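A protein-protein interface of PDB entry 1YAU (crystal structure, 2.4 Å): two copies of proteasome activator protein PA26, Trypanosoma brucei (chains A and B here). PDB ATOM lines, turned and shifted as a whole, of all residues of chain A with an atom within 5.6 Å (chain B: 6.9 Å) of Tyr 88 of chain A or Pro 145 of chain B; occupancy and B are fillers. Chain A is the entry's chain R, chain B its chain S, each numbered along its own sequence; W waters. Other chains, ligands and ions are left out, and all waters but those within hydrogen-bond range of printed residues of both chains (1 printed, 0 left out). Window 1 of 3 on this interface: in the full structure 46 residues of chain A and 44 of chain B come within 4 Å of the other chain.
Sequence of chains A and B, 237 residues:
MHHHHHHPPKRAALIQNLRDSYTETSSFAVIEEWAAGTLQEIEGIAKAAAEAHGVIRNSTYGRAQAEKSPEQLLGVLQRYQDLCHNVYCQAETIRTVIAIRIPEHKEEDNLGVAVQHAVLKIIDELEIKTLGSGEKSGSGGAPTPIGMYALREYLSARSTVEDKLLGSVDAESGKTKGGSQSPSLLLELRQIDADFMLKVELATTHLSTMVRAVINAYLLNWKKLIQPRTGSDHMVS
The backbone NH (N) of Glu 135 of chain A sits at hydrogen-bond distance from the backbone carbonyl oxygen (O) of Ala 142 of chain B (2.8 Å).
The side-chain carboxylate (OE2) of Glu 92 of chain A sits at hydrogen-bond distance from a ring nitrogen (ND1) of His 206 of chain B (3.0 Å).
The backbone NH (N) of Glu 135 of chain A sits at hydrogen-bond distance from the backbone carbonyl oxygen (O) of Thr 144 of chain B.
The side-chain carboxylate of Glu 153 of chain B lies close to the side-chain carboxylate of Glu 135 of chain A.
NE2 of His 85 of chain A sits close to OE2 of Glu 201 of chain B, at 3.5 Å.
The backbone carbonyl oxygen (O) of Glu 127 of chain A sits at hydrogen-bond distance from the side-chain hydroxyl (OG) of Ser 133 of chain A (2.8 Å).
The side-chain sulfur (SD) of Met 148 of chain A sits at hydrogen-bond distance from the backbone NH (N) of His 85 of chain A (3.6 Å).
The side-chain hydroxyl (OG1) of Thr 204 of chain B lies within hydrogen-bond range of the backbone carbonyl oxygen (O) of Glu 201 of chain B (3.0 Å).
Leu 198 of chain B touches His 85 of chain A.
Pro 145 of chain B touches Tyr 88 of chain A.
Tyr 88 of chain A touches Leu 202 of chain B.
Tyr 88 of chain A touches His 206 of chain B (OH to CB, 3.4 Å).
CA of Gly 134 of chain A touches O of Thr 144 of chain B, 3.7 Å away.
OE1 of Glu 135 of chain A touches N of Gly 147 of chain B, at 3.8 Å.
CD1 of Leu 202 of chain B touches SD of Met 148 of chain A (3.8 Å).
Tyr 149 of chain A touches Pro 145 of chain B.
Leu 202 of chain B touches Tyr 149 of chain A (CD1 to OH, 3.8 Å).
Printed residues of chain B within 4 Å of Tyr 88 of chain A: Pro 145, Leu 202 and His 206.
Of the printed residues of chain A, Thr 144 of chain B touches Gly 134 and Glu 135.
Of chain A, only Tyr 88 (3.8 Å), Ser 133 (3.5 Å), Glu 135 (3.2 Å) and Tyr 149 (3.6 Å) come within 4 Å of Pro 145 of chain B.
Of the printed residues of chain A, Glu 201 of chain B touches His 85.
Printed residues of chain A within 4 Å of His 206 of chain B: Tyr 88 (3.4 Å) and Glu 92 (3.0 Å).
The nearest residue of chain A that does not touch Pro 145 of chain B is Gly 134 of chain A (4.5 Å).
The nearest printed residue of chain A that does not touch Leu 198 of chain B is Met 148 of chain A (4.1 Å).
Of the 20 printed residues of chain B, 12 touch a printed residue of chain A.
Hydrophobic or aromatic side chains of chain B within 4 Å of the printed part of chain A: Ala 142, Pro 143, Pro 145, Leu 198, Leu 202 and His 206.
Of the 19 printed residues of chain A, 9 touch a printed residue of chain B.
Printed residues of chain A that touch a printed residue of chain B: His 85, Tyr 88, Glu 92, Ile 128, Ser 133, Gly 134, Glu 135, Met 148 and Tyr 149.
Among the printed residues, 23 pairs touch across the chains.
No position is printed for both chains.
Water W1 bridges the side-chain carboxylate of Asp 195 of chain B and the backbone carbonyl oxygen of Tyr 149 of chain A.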
ATOM      1  N   LEU A  83      16.304 -22.456 -33.658  1.00  0.00           N
ATOM      2  CA  LEU A  83      17.283 -21.582 -34.238  1.00  0.00           C
ATOM      3  C   LEU A  83      17.765 -20.572 -33.148  1.00  0.00           C
ATOM      4  O   LEU A  83      18.949 -20.488 -32.868  1.00  0.00           O
ATOM      5  CB  LEU A  83      16.749 -20.889 -35.504  1.00  0.00           C
ATOM      6  CG  LEU A  83      17.892 -19.976 -35.997  1.00  0.00           C
ATOM      7  CD1 LEU A  83      18.539 -20.531 -37.233  1.00  0.00           C
ATOM      8  CD2 LEU A  83      17.449 -18.549 -36.180  1.00  0.00           C
ATOM      9  N   CYS A  84      16.825 -19.830 -32.553  1.00  0.00           N
ATOM     10  CA  CYS A  84      17.135 -18.878 -31.480  1.00  0.00           C
ATOM     11  C   CYS A  84      18.007 -19.479 -30.374  1.00  0.00           C
ATOM     12  O   CYS A  84      18.994 -18.876 -29.960  1.00  0.00           O
ATOM     13  CB  CYS A  84      15.845 -18.333 -30.908  1.00  0.00           C
ATOM     14  SG  CYS A  84      15.030 -17.290 -32.111  1.00  0.00           S
ATOM     15  N   HIS A  85      17.652 -20.685 -29.939  1.00  0.00           N
ATOM     16  CA  HIS A  85      18.389 -21.417 -28.920  1.00  0.00           C
ATOM     17  C   HIS A  85      19.846 -21.576 -29.303  1.00  0.00           C
ATOM     18  O   HIS A  85      20.731 -21.290 -28.484  1.00  0.00           O
ATOM     19  CB  HIS A  85      17.720 -22.773 -28.657  1.00  0.00           C
ATOM     20  CG  HIS A  85      18.534 -23.730 -27.829  1.00  0.00           C
ATOM     21  ND1 HIS A  85      18.284 -25.086 -27.813  1.00  0.00           N
ATOM     22  CD2 HIS A  85      19.578 -23.536 -26.991  1.00  0.00           C
ATOM     23  CE1 HIS A  85      19.145 -25.685 -27.013  1.00  0.00           C
ATOM     24  NE2 HIS A  85      19.941 -24.766 -26.498  1.00  0.00           N
ATOM     25  N   ASN A  86      20.107 -22.055 -30.518  1.00  0.00           N
ATOM     26  CA  ASN A  86      21.494 -22.205 -30.941  1.00  0.00           C
ATOM     27  C   ASN A  86      22.258 -20.864 -31.081  1.00  0.00           C
ATOM     28  O   ASN A  86      23.446 -20.801 -30.774  1.00  0.00           O
ATOM     29  CB  ASN A  86      21.606 -22.982 -32.268  1.00  0.00           C
ATOM     30  CG  ASN A  86      20.842 -24.303 -32.266  1.00  0.00           C
ATOM     31  OD1 ASN A  86      20.858 -25.082 -31.297  1.00  0.00           O
ATOM     32  ND2 ASN A  86      20.160 -24.559 -33.374  1.00  0.00           N
ATOM     33  N   VAL A  87      21.601 -19.832 -31.617  1.00  0.00           N
ATOM     34  CA  VAL A  87      22.248 -18.522 -31.798  1.00  0.00           C
ATOM     35  C   VAL A  87      22.665 -17.971 -30.428  1.00  0.00           C
ATOM     36  O   VAL A  87      23.809 -17.551 -30.242  1.00  0.00           O
ATOM     37  CB  VAL A  87      21.368 -17.512 -32.607  1.00  0.00           C
ATOM     38  CG1 VAL A  87      21.972 -16.111 -32.609  1.00  0.00           C
ATOM     39  CG2 VAL A  87      21.206 -17.993 -34.042  1.00  0.00           C
ATOM     40  N   TYR A  88      21.751 -18.056 -29.468  1.00  0.00           N
ATOM     41  CA  TYR A  88      22.026 -17.724 -28.081  1.00  0.00           C
ATOM     42  C   TYR A  88      23.285 -18.402 -27.530  1.00  0.00           C
ATOM     43  O   TYR A  88      24.177 -17.710 -26.986  1.00  0.00           O
ATOM     44  CB  TYR A  88      20.800 -18.065 -27.220  1.00  0.00           C
ATOM     45  CG  TYR A  88      20.923 -17.593 -25.802  1.00  0.00           C
ATOM     46  CD1 TYR A  88      20.450 -16.336 -25.434  1.00  0.00           C
ATOM     47  CD2 TYR A  88      21.543 -18.389 -24.830  1.00  0.00           C
ATOM     48  CE1 TYR A  88      20.576 -15.871 -24.131  1.00  0.00           C
ATOM     49  CE2 TYR A  88      21.682 -17.952 -23.529  1.00  0.00           C
ATOM     50  CZ  TYR A  88      21.182 -16.687 -23.181  1.00  0.00           C
ATOM     51  OH  TYR A  88      21.289 -16.238 -21.892  1.00  0.00           O
ATOM     52  N   CYS A  89      23.348 -19.743 -27.626  1.00  0.00           N
ATOM     53  CA  CYS A  89      24.485 -20.503 -27.077  1.00  0.00           C
ATOM     54  C   CYS A  89      25.809 -20.133 -27.772  1.00  0.00           C
ATOM     55  O   CYS A  89      26.883 -20.093 -27.144  1.00  0.00           O
ATOM     56  CB  CYS A  89      24.225 -22.018 -27.150  1.00  0.00           C
ATOM     57  SG  CYS A  89      22.906 -22.578 -26.008  1.00  0.00           S
ATOM     58  N   GLN A  90      25.714 -19.849 -29.068  1.00  0.00           N
ATOM     59  CA  GLN A  90      26.858 -19.459 -29.877  1.00  0.00           C
ATOM     60  C   GLN A  90      27.338 -18.019 -29.544  1.00  0.00           C
ATOM     61  O   GLN A  90      28.559 -17.771 -29.438  1.00  0.00           O
ATOM     62  CB  GLN A  90      26.517 -19.619 -31.380  1.00  0.00           C
ATOM     63  CG  GLN A  90      26.471 -21.084 -31.846  1.00  0.00           C
ATOM     64  CD  GLN A  90      25.753 -21.272 -33.205  1.00  0.00           C
ATOM     65  OE1 GLN A  90      24.880 -20.489 -33.603  1.00  0.00           O
ATOM     66  NE2 GLN A  90      26.127 -22.313 -33.901  1.00  0.00           N
ATOM     67  N   ALA A  91      26.376 -17.091 -29.406  1.00  0.00           N
ATOM     68  CA  ALA A  91      26.627 -15.752 -28.825  1.00  0.00           C
ATOM     69  C   ALA A  91      27.383 -15.855 -27.503  1.00  0.00           C
ATOM     70  O   ALA A  91      28.356 -15.166 -27.305  1.00  0.00           O
ATOM     71  CB  ALA A  91      25.356 -15.009 -28.618  1.00  0.00           C
ATOM     72  N   GLU A  92      26.976 -16.770 -26.630  1.00  0.00           N
ATOM     73  CA  GLU A  92      27.609 -16.892 -25.338  1.00  0.00           C
ATOM     74  C   GLU A  92      29.021 -17.324 -25.444  1.00  0.00           C
ATOM     75  O   GLU A  92      29.831 -16.991 -24.580  1.00  0.00           O
ATOM     76  CB  GLU A  92      26.827 -17.831 -24.421  1.00  0.00           C
ATOM     77  CG  GLU A  92      25.482 -17.246 -23.980  1.00  0.00           C
ATOM     78  CD  GLU A  92      25.658 -16.145 -22.942  1.00  0.00           C
ATOM     79  OE1 GLU A  92      26.564 -16.223 -22.080  1.00  0.00           O
ATOM     80  OE2 GLU A  92      24.878 -15.193 -22.960  1.00  0.00           O
ATOM     81  N   THR A  93      29.340 -18.091 -26.488  1.00  0.00           N
ATOM     82  CA  THR A  93      30.737 -18.493 -26.734  1.00  0.00           C
ATOM     83  C   THR A  93      31.584 -17.268 -26.996  1.00  0.00           C
ATOM     84  O   THR A  93      32.664 -17.133 -26.425  1.00  0.00           O
ATOM     85  CB  THR A  93      30.848 -19.492 -27.894  1.00  0.00           C
ATOM     86  OG1 THR A  93      30.523 -20.779 -27.384  1.00  0.00           O
ATOM     87  CG2 THR A  93      32.342 -19.644 -28.395  1.00  0.00           C
ATOM     88  N   GLU A 127      21.161 -11.162 -27.949  1.00  0.00           N
ATOM     89  CA  GLU A 127      20.625 -12.178 -27.042  1.00  0.00           C
ATOM     90  C   GLU A 127      19.366 -11.690 -26.334  1.00  0.00           C
ATOM     91  O   GLU A 127      18.375 -12.415 -26.260  1.00  0.00           O
ATOM     92  CB  GLU A 127      21.668 -12.599 -26.001  1.00  0.00           C
ATOM     93  CG  GLU A 127      23.039 -13.004 -26.519  1.00  0.00           C
ATOM     94  CD  GLU A 127      23.821 -13.827 -25.499  1.00  0.00           C
ATOM     95  OE1 GLU A 127      23.242 -14.702 -24.877  1.00  0.00           O
ATOM     96  OE2 GLU A 127      25.019 -13.648 -25.289  1.00  0.00           O
ATOM     97  N   ILE A 128      19.411 -10.456 -25.823  1.00  0.00           N
ATOM     98  CA  ILE A 128      18.340  -9.912 -24.986  1.00  0.00           C
ATOM     99  C   ILE A 128      17.223  -9.376 -25.854  1.00  0.00           C
ATOM    100  O   ILE A 128      16.111  -9.897 -25.829  1.00  0.00           O
ATOM    101  CB  ILE A 128      18.866  -8.802 -23.981  1.00  0.00           C
ATOM    102  CG1 ILE A 128      19.973  -9.329 -23.018  1.00  0.00           C
ATOM    103  CG2 ILE A 128      17.695  -8.082 -23.250  1.00  0.00           C
ATOM    104  CD1 ILE A 128      19.745 -10.734 -22.440  1.00  0.00           C
ATOM    105  N   LEU A 131      16.617 -11.885 -29.656  1.00  0.00           N
ATOM    106  CA  LEU A 131      16.175 -13.248 -29.386  1.00  0.00           C
ATOM    107  C   LEU A 131      15.179 -13.356 -28.228  1.00  0.00           C
ATOM    108  O   LEU A 131      14.731 -14.457 -27.909  1.00  0.00           O
ATOM    109  CB  LEU A 131      17.356 -14.155 -29.076  1.00  0.00           C
ATOM    110  CG  LEU A 131      18.448 -14.413 -30.099  1.00  0.00           C
ATOM    111  CD1 LEU A 131      19.414 -15.354 -29.475  1.00  0.00           C
ATOM    112  CD2 LEU A 131      17.916 -14.994 -31.391  1.00  0.00           C
ATOM    113  N   SER A 133      15.345 -13.605 -25.166  1.00  0.00           N
ATOM    114  CA  SER A 133      15.742 -14.740 -24.344  1.00  0.00           C
ATOM    115  C   SER A 133      15.442 -14.594 -22.858  1.00  0.00           C
ATOM    116  O   SER A 133      15.375 -15.602 -22.139  1.00  0.00           O
ATOM    117  CB  SER A 133      17.234 -14.982 -24.489  1.00  0.00           C
ATOM    118  OG  SER A 133      17.951 -13.921 -23.888  1.00  0.00           O
ATOM    119  N   GLY A 134      15.309 -13.345 -22.401  1.00  0.00           N
ATOM    120  CA  GLY A 134      15.099 -13.039 -20.988  1.00  0.00           C
ATOM    121  C   GLY A 134      13.692 -13.305 -20.491  1.00  0.00           C
ATOM    122  O   GLY A 134      12.723 -13.151 -21.233  1.00  0.00           O
ATOM    123  N   GLU A 135      13.596 -13.709 -19.225  1.00  0.00           N
ATOM    124  CA  GLU A 135      12.324 -13.848 -18.497  1.00  0.00           C
ATOM    125  C   GLU A 135      11.401 -12.632 -18.607  1.00  0.00           C
ATOM    126  O   GLU A 135      10.185 -12.769 -18.779  1.00  0.00           O
ATOM    127  CB  GLU A 135      12.607 -14.064 -17.022  1.00  0.00           C
ATOM    128  CG  GLU A 135      12.381 -15.472 -16.515  1.00  0.00           C
ATOM    129  CD  GLU A 135      12.483 -15.534 -15.001  1.00  0.00           C
ATOM    130  OE1 GLU A 135      13.373 -14.865 -14.421  1.00  0.00           O
ATOM    131  OE2 GLU A 135      11.671 -16.250 -14.393  1.00  0.00           O
ATOM    132  N   MET A 148      12.099 -16.074 -28.044  1.00  0.00           N
ATOM    133  CA  MET A 148      12.462 -17.474 -27.891  1.00  0.00           C
ATOM    134  C   MET A 148      11.293 -18.407 -27.504  1.00  0.00           C
ATOM    135  O   MET A 148      11.331 -19.592 -27.797  1.00  0.00           O
ATOM    136  CB  MET A 148      13.562 -17.561 -26.815  1.00  0.00           C
ATOM    137  CG  MET A 148      14.068 -18.963 -26.453  1.00  0.00           C
ATOM    138  SD  MET A 148      15.631 -19.364 -27.256  1.00  0.00           S
ATOM    139  CE  MET A 148      16.520 -17.808 -27.022  1.00  0.00           C
ATOM    140  N   TYR A 149      10.291 -17.879 -26.806  1.00  0.00           N
ATOM    141  CA  TYR A 149       9.211 -18.690 -26.234  1.00  0.00           C
ATOM    142  C   TYR A 149       7.928 -18.368 -26.978  1.00  0.00           C
ATOM    143  O   TYR A 149       6.841 -18.295 -26.391  1.00  0.00           O
ATOM    144  CB  TYR A 149       9.094 -18.454 -24.709  1.00  0.00           C
ATOM    145  CG  TYR A 149      10.467 -18.421 -24.080  1.00  0.00           C
ATOM    146  CD1 TYR A 149      11.044 -17.196 -23.675  1.00  0.00           C
ATOM    147  CD2 TYR A 149      11.237 -19.593 -23.972  1.00  0.00           C
ATOM    148  CE1 TYR A 149      12.333 -17.153 -23.146  1.00  0.00           C
ATOM    149  CE2 TYR A 149      12.526 -19.558 -23.451  1.00  0.00           C
ATOM    150  CZ  TYR A 149      13.062 -18.333 -23.037  1.00  0.00           C
ATOM    151  OH  TYR A 149      14.329 -18.282 -22.526  1.00  0.00           O
ATOM    152  N   THR B 130      21.963 -12.295 -13.239  1.00  0.00           N
ATOM    153  CA  THR B 130      22.214 -13.673 -13.635  1.00  0.00           C
ATOM    154  C   THR B 130      21.455 -14.698 -12.744  1.00  0.00           C
ATOM    155  O   THR B 130      20.764 -15.595 -13.253  1.00  0.00           O
ATOM    156  CB  THR B 130      23.744 -13.930 -13.684  1.00  0.00           C
ATOM    157  OG1 THR B 130      24.397 -12.858 -14.383  1.00  0.00           O
ATOM    158  CG2 THR B 130      24.086 -15.163 -14.511  1.00  0.00           C
ATOM    159  N   ALA B 142      14.228  -8.968 -16.256  1.00  0.00           N
ATOM    160  CA  ALA B 142      15.044 -10.170 -16.027  1.00  0.00           C
ATOM    161  C   ALA B 142      15.545 -10.754 -17.365  1.00  0.00           C
ATOM    162  O   ALA B 142      14.792 -11.423 -18.093  1.00  0.00           O
ATOM    163  CB  ALA B 142      14.264 -11.216 -15.226  1.00  0.00           C
ATOM    164  N   PRO B 143      16.816 -10.500 -17.684  1.00  0.00           N
ATOM    165  CA  PRO B 143      17.364 -10.837 -18.996  1.00  0.00           C
ATOM    166  C   PRO B 143      17.933 -12.270 -19.019  1.00  0.00           C
ATOM    167  O   PRO B 143      18.350 -12.780 -20.077  1.00  0.00           O
ATOM    168  CB  PRO B 143      18.473  -9.783 -19.183  1.00  0.00           C
ATOM    169  CG  PRO B 143      18.625  -9.089 -17.807  1.00  0.00           C
ATOM    170  CD  PRO B 143      17.842  -9.893 -16.815  1.00  0.00           C
ATOM    171  N   THR B 144      17.940 -12.905 -17.848  1.00  0.00           N
ATOM    172  CA  THR B 144      18.301 -14.300 -17.743  1.00  0.00           C
ATOM    173  C   THR B 144      17.051 -15.131 -18.077  1.00  0.00           C
ATOM    174  O   THR B 144      15.925 -14.698 -17.790  1.00  0.00           O
ATOM    175  CB  THR B 144      18.950 -14.609 -16.356  1.00  0.00           C
ATOM    176  OG1 THR B 144      19.734 -15.817 -16.435  1.00  0.00           O
ATOM    177  CG2 THR B 144      17.888 -14.847 -15.244  1.00  0.00           C
ATOM    178  N   PRO B 145      17.238 -16.262 -18.771  1.00  0.00           N
ATOM    179  CA  PRO B 145      16.106 -17.157 -19.117  1.00  0.00           C
ATOM    180  C   PRO B 145      15.269 -17.642 -17.924  1.00  0.00           C
ATOM    181  O   PRO B 145      14.053 -17.720 -18.045  1.00  0.00           O
ATOM    182  CB  PRO B 145      16.789 -18.306 -19.841  1.00  0.00           C
ATOM    183  CG  PRO B 145      18.003 -17.615 -20.458  1.00  0.00           C
ATOM    184  CD  PRO B 145      18.512 -16.740 -19.358  1.00  0.00           C
ATOM    185  N   ILE B 146      15.916 -17.912 -16.789  1.00  0.00           N
ATOM    186  CA  ILE B 146      15.261 -18.444 -15.577  1.00  0.00           C
ATOM    187  C   ILE B 146      16.051 -18.009 -14.340  1.00  0.00           C
ATOM    188  O   ILE B 146      17.240 -17.783 -14.438  1.00  0.00           O
ATOM    189  CB  ILE B 146      15.137 -20.023 -15.669  1.00  0.00           C
ATOM    190  CG1 ILE B 146      13.985 -20.551 -14.822  1.00  0.00           C
ATOM    191  CG2 ILE B 146      16.417 -20.741 -15.277  1.00  0.00           C
ATOM    192  CD1 ILE B 146      12.635 -20.052 -15.253  1.00  0.00           C
ATOM    193  N   GLY B 147      15.407 -17.888 -13.185  1.00  0.00           N
ATOM    194  CA  GLY B 147      16.136 -17.570 -11.957  1.00  0.00           C
ATOM    195  C   GLY B 147      16.163 -18.643 -10.873  1.00  0.00           C
ATOM    196  O   GLY B 147      15.637 -19.734 -11.060  1.00  0.00           O
ATOM    197  N   GLU B 153       8.335 -21.267 -10.027  1.00  0.00           N
ATOM    198  CA  GLU B 153       7.795 -20.705 -11.280  1.00  0.00           C
ATOM    199  C   GLU B 153       7.282 -21.821 -12.206  1.00  0.00           C
ATOM    200  O   GLU B 153       6.259 -21.665 -12.851  1.00  0.00           O
ATOM    201  CB  GLU B 153       8.838 -19.930 -12.107  1.00  0.00           C
ATOM    202  CG  GLU B 153       9.743 -18.881 -11.463  1.00  0.00           C
ATOM    203  CD  GLU B 153      10.749 -18.340 -12.507  1.00  0.00           C
ATOM    204  OE1 GLU B 153      11.901 -17.932 -12.155  1.00  0.00           O
ATOM    205  OE2 GLU B 153      10.390 -18.364 -13.730  1.00  0.00           O
ATOM    206  N   ASP B 195       9.887 -25.863 -22.325  1.00  0.00           N
ATOM    207  CA  ASP B 195      10.440 -24.498 -22.181  1.00  0.00           C
ATOM    208  C   ASP B 195      11.168 -24.288 -20.884  1.00  0.00           C
ATOM    209  O   ASP B 195      12.128 -23.553 -20.867  1.00  0.00           O
ATOM    210  CB  ASP B 195       9.374 -23.425 -22.334  1.00  0.00           C
ATOM    211  CG  ASP B 195       9.052 -23.136 -23.760  1.00  0.00           C
ATOM    212  OD1 ASP B 195       9.691 -23.723 -24.663  1.00  0.00           O
ATOM    213  OD2 ASP B 195       8.168 -22.316 -24.076  1.00  0.00           O
ATOM    214  N   PHE B 196      10.744 -24.959 -19.816  1.00  0.00           N
ATOM    215  CA  PHE B 196      11.484 -24.901 -18.559  1.00  0.00           C
ATOM    216  C   PHE B 196      12.826 -25.603 -18.575  1.00  0.00           C
ATOM    217  O   PHE B 196      13.766 -25.123 -17.918  1.00  0.00           O
ATOM    218  CB  PHE B 196      10.620 -25.267 -17.347  1.00  0.00           C
ATOM    219  CG  PHE B 196       9.883 -24.085 -16.808  1.00  0.00           C
ATOM    220  CD1 PHE B 196       8.699 -23.653 -17.419  1.00  0.00           C
ATOM    221  CD2 PHE B 196      10.435 -23.311 -15.771  1.00  0.00           C
ATOM    222  CE1 PHE B 196       8.031 -22.516 -16.949  1.00  0.00           C
ATOM    223  CE2 PHE B 196       9.791 -22.143 -15.320  1.00  0.00           C
ATOM    224  CZ  PHE B 196       8.602 -21.748 -15.890  1.00  0.00           C
ATOM    225  N   LEU B 198      14.510 -25.903 -21.499  1.00  0.00           N
ATOM    226  CA  LEU B 198      15.251 -25.011 -22.374  1.00  0.00           C
ATOM    227  C   LEU B 198      15.829 -23.829 -21.579  1.00  0.00           C
ATOM    228  O   LEU B 198      17.015 -23.505 -21.734  1.00  0.00           O
ATOM    229  CB  LEU B 198      14.393 -24.526 -23.533  1.00  0.00           C
ATOM    230  CG  LEU B 198      14.991 -23.429 -24.455  1.00  0.00           C
ATOM    231  CD1 LEU B 198      16.169 -23.929 -25.283  1.00  0.00           C
ATOM    232  CD2 LEU B 198      13.928 -22.924 -25.372  1.00  0.00           C
ATOM    233  N   LYS B 199      14.998 -23.228 -20.713  1.00  0.00           N
ATOM    234  CA  LYS B 199      15.390 -22.106 -19.851  1.00  0.00           C
ATOM    235  C   LYS B 199      16.582 -22.433 -18.969  1.00  0.00           C
ATOM    236  O   LYS B 199      17.478 -21.618 -18.843  1.00  0.00           O
ATOM    237  CB  LYS B 199      14.191 -21.608 -18.998  1.00  0.00           C
ATOM    238  CG  LYS B 199      13.065 -21.027 -19.842  1.00  0.00           C
ATOM    239  CD  LYS B 199      11.857 -20.510 -19.027  1.00  0.00           C
ATOM    240  CE  LYS B 199      11.177 -19.426 -19.889  1.00  0.00           C
ATOM    241  NZ  LYS B 199       9.962 -18.797 -19.307  1.00  0.00           N
ATOM    242  N   VAL B 200      16.592 -23.621 -18.364  1.00  0.00           N
ATOM    243  CA  VAL B 200      17.761 -24.118 -17.607  1.00  0.00           C
ATOM    244  C   VAL B 200      19.033 -24.241 -18.452  1.00  0.00           C
ATOM    245  O   VAL B 200      20.132 -23.877 -17.962  1.00  0.00           O
ATOM    246  CB  VAL B 200      17.516 -25.498 -16.927  1.00  0.00           C
ATOM    247  CG1 VAL B 200      18.768 -25.953 -16.214  1.00  0.00           C
ATOM    248  CG2 VAL B 200      16.388 -25.418 -15.950  1.00  0.00           C
ATOM    249  N   GLU B 201      18.910 -24.785 -19.674  1.00  0.00           N
ATOM    250  CA  GLU B 201      20.072 -24.890 -20.601  1.00  0.00           C
ATOM    251  C   GLU B 201      20.686 -23.514 -20.920  1.00  0.00           C
ATOM    252  O   GLU B 201      21.911 -23.378 -20.945  1.00  0.00           O
ATOM    253  CB  GLU B 201      19.680 -25.457 -21.960  1.00  0.00           C
ATOM    254  CG  GLU B 201      18.895 -26.733 -21.948  1.00  0.00           C
ATOM    255  CD  GLU B 201      18.794 -27.318 -23.349  1.00  0.00           C
ATOM    256  OE1 GLU B 201      17.678 -27.778 -23.683  1.00  0.00           O
ATOM    257  OE2 GLU B 201      19.826 -27.295 -24.096  1.00  0.00           O
ATOM    258  N   LEU B 202      19.801 -22.545 -21.225  1.00  0.00           N
ATOM    259  CA  LEU B 202      20.197 -21.209 -21.574  1.00  0.00           C
ATOM    260  C   LEU B 202      20.769 -20.528 -20.331  1.00  0.00           C
ATOM    261  O   LEU B 202      21.869 -20.001 -20.390  1.00  0.00           O
ATOM    262  CB  LEU B 202      19.040 -20.409 -22.191  1.00  0.00           C
ATOM    263  CG  LEU B 202      18.445 -20.931 -23.510  1.00  0.00           C
ATOM    264  CD1 LEU B 202      17.314 -20.070 -23.942  1.00  0.00           C
ATOM    265  CD2 LEU B 202      19.453 -20.997 -24.643  1.00  0.00           C
ATOM    266  N   ALA B 203      20.063 -20.602 -19.202  1.00  0.00           N
ATOM    267  CA  ALA B 203      20.502 -19.938 -17.976  1.00  0.00           C
ATOM    268  C   ALA B 203      21.863 -20.448 -17.491  1.00  0.00           C
ATOM    269  O   ALA B 203      22.722 -19.622 -17.160  1.00  0.00           O
ATOM    270  CB  ALA B 203      19.475 -20.047 -16.909  1.00  0.00           C
ATOM    271  N   THR B 204      22.090 -21.773 -17.478  1.00  0.00           N
ATOM    272  CA  THR B 204      23.418 -22.347 -17.122  1.00  0.00           C
ATOM    273  C   THR B 204      24.519 -21.883 -18.054  1.00  0.00           C
ATOM    274  O   THR B 204      25.671 -21.700 -17.616  1.00  0.00           O
ATOM    275  CB  THR B 204      23.434 -23.923 -17.107  1.00  0.00           C
ATOM    276  OG1 THR B 204      22.810 -24.423 -18.291  1.00  0.00           O
ATOM    277  CG2 THR B 204      22.561 -24.478 -15.983  1.00  0.00           C
ATOM    278  N   THR B 205      24.184 -21.685 -19.321  1.00  0.00           N
ATOM    279  CA  THR B 205      25.149 -21.157 -20.279  1.00  0.00           C
ATOM    280  C   THR B 205      25.515 -19.708 -19.940  1.00  0.00           C
ATOM    281  O   THR B 205      26.679 -19.398 -19.782  1.00  0.00           O
ATOM    282  CB  THR B 205      24.600 -21.209 -21.723  1.00  0.00           C
ATOM    283  OG1 THR B 205      24.253 -22.556 -22.034  1.00  0.00           O
ATOM    284  CG2 THR B 205      25.694 -20.874 -22.709  1.00  0.00           C
ATOM    285  N   HIS B 206      24.514 -18.836 -19.860  1.00  0.00           N
ATOM    286  CA  HIS B 206      24.726 -17.465 -19.394  1.00  0.00           C
ATOM    287  C   HIS B 206      25.505 -17.394 -18.069  1.00  0.00           C
ATOM    288  O   HIS B 206      26.427 -16.624 -17.912  1.00  0.00           O
ATOM    289  CB  HIS B 206      23.415 -16.740 -19.254  1.00  0.00           C
ATOM    290  CG  HIS B 206      23.600 -15.271 -19.123  1.00  0.00           C
ATOM    291  ND1 HIS B 206      23.922 -14.469 -20.203  1.00  0.00           N
ATOM    292  CD2 HIS B 206      23.605 -14.467 -18.034  1.00  0.00           C
ATOM    293  CE1 HIS B 206      24.078 -13.226 -19.786  1.00  0.00           C
ATOM    294  NE2 HIS B 206      23.910 -13.201 -18.474  1.00  0.00           N
ATOM    295  N   LEU B 207      25.171 -18.268 -17.145  1.00  0.00           N
ATOM    296  CA  LEU B 207      25.796 -18.249 -15.870  1.00  0.00           C
ATOM    297  C   LEU B 207      27.273 -18.702 -15.925  1.00  0.00           C
ATOM    298  O   LEU B 207      28.129 -18.183 -15.190  1.00  0.00           O
ATOM    299  CB  LEU B 207      24.964 -19.105 -14.911  1.00  0.00           C
ATOM    300  CG  LEU B 207      25.583 -19.345 -13.557  1.00  0.00           C
ATOM    301  CD1 LEU B 207      25.690 -18.044 -12.732  1.00  0.00           C
ATOM    302  CD2 LEU B 207      24.792 -20.415 -12.822  1.00  0.00           C
HETATM  303  O   HOH W   1       7.996 -21.579 -26.493  1.00  0.00           O
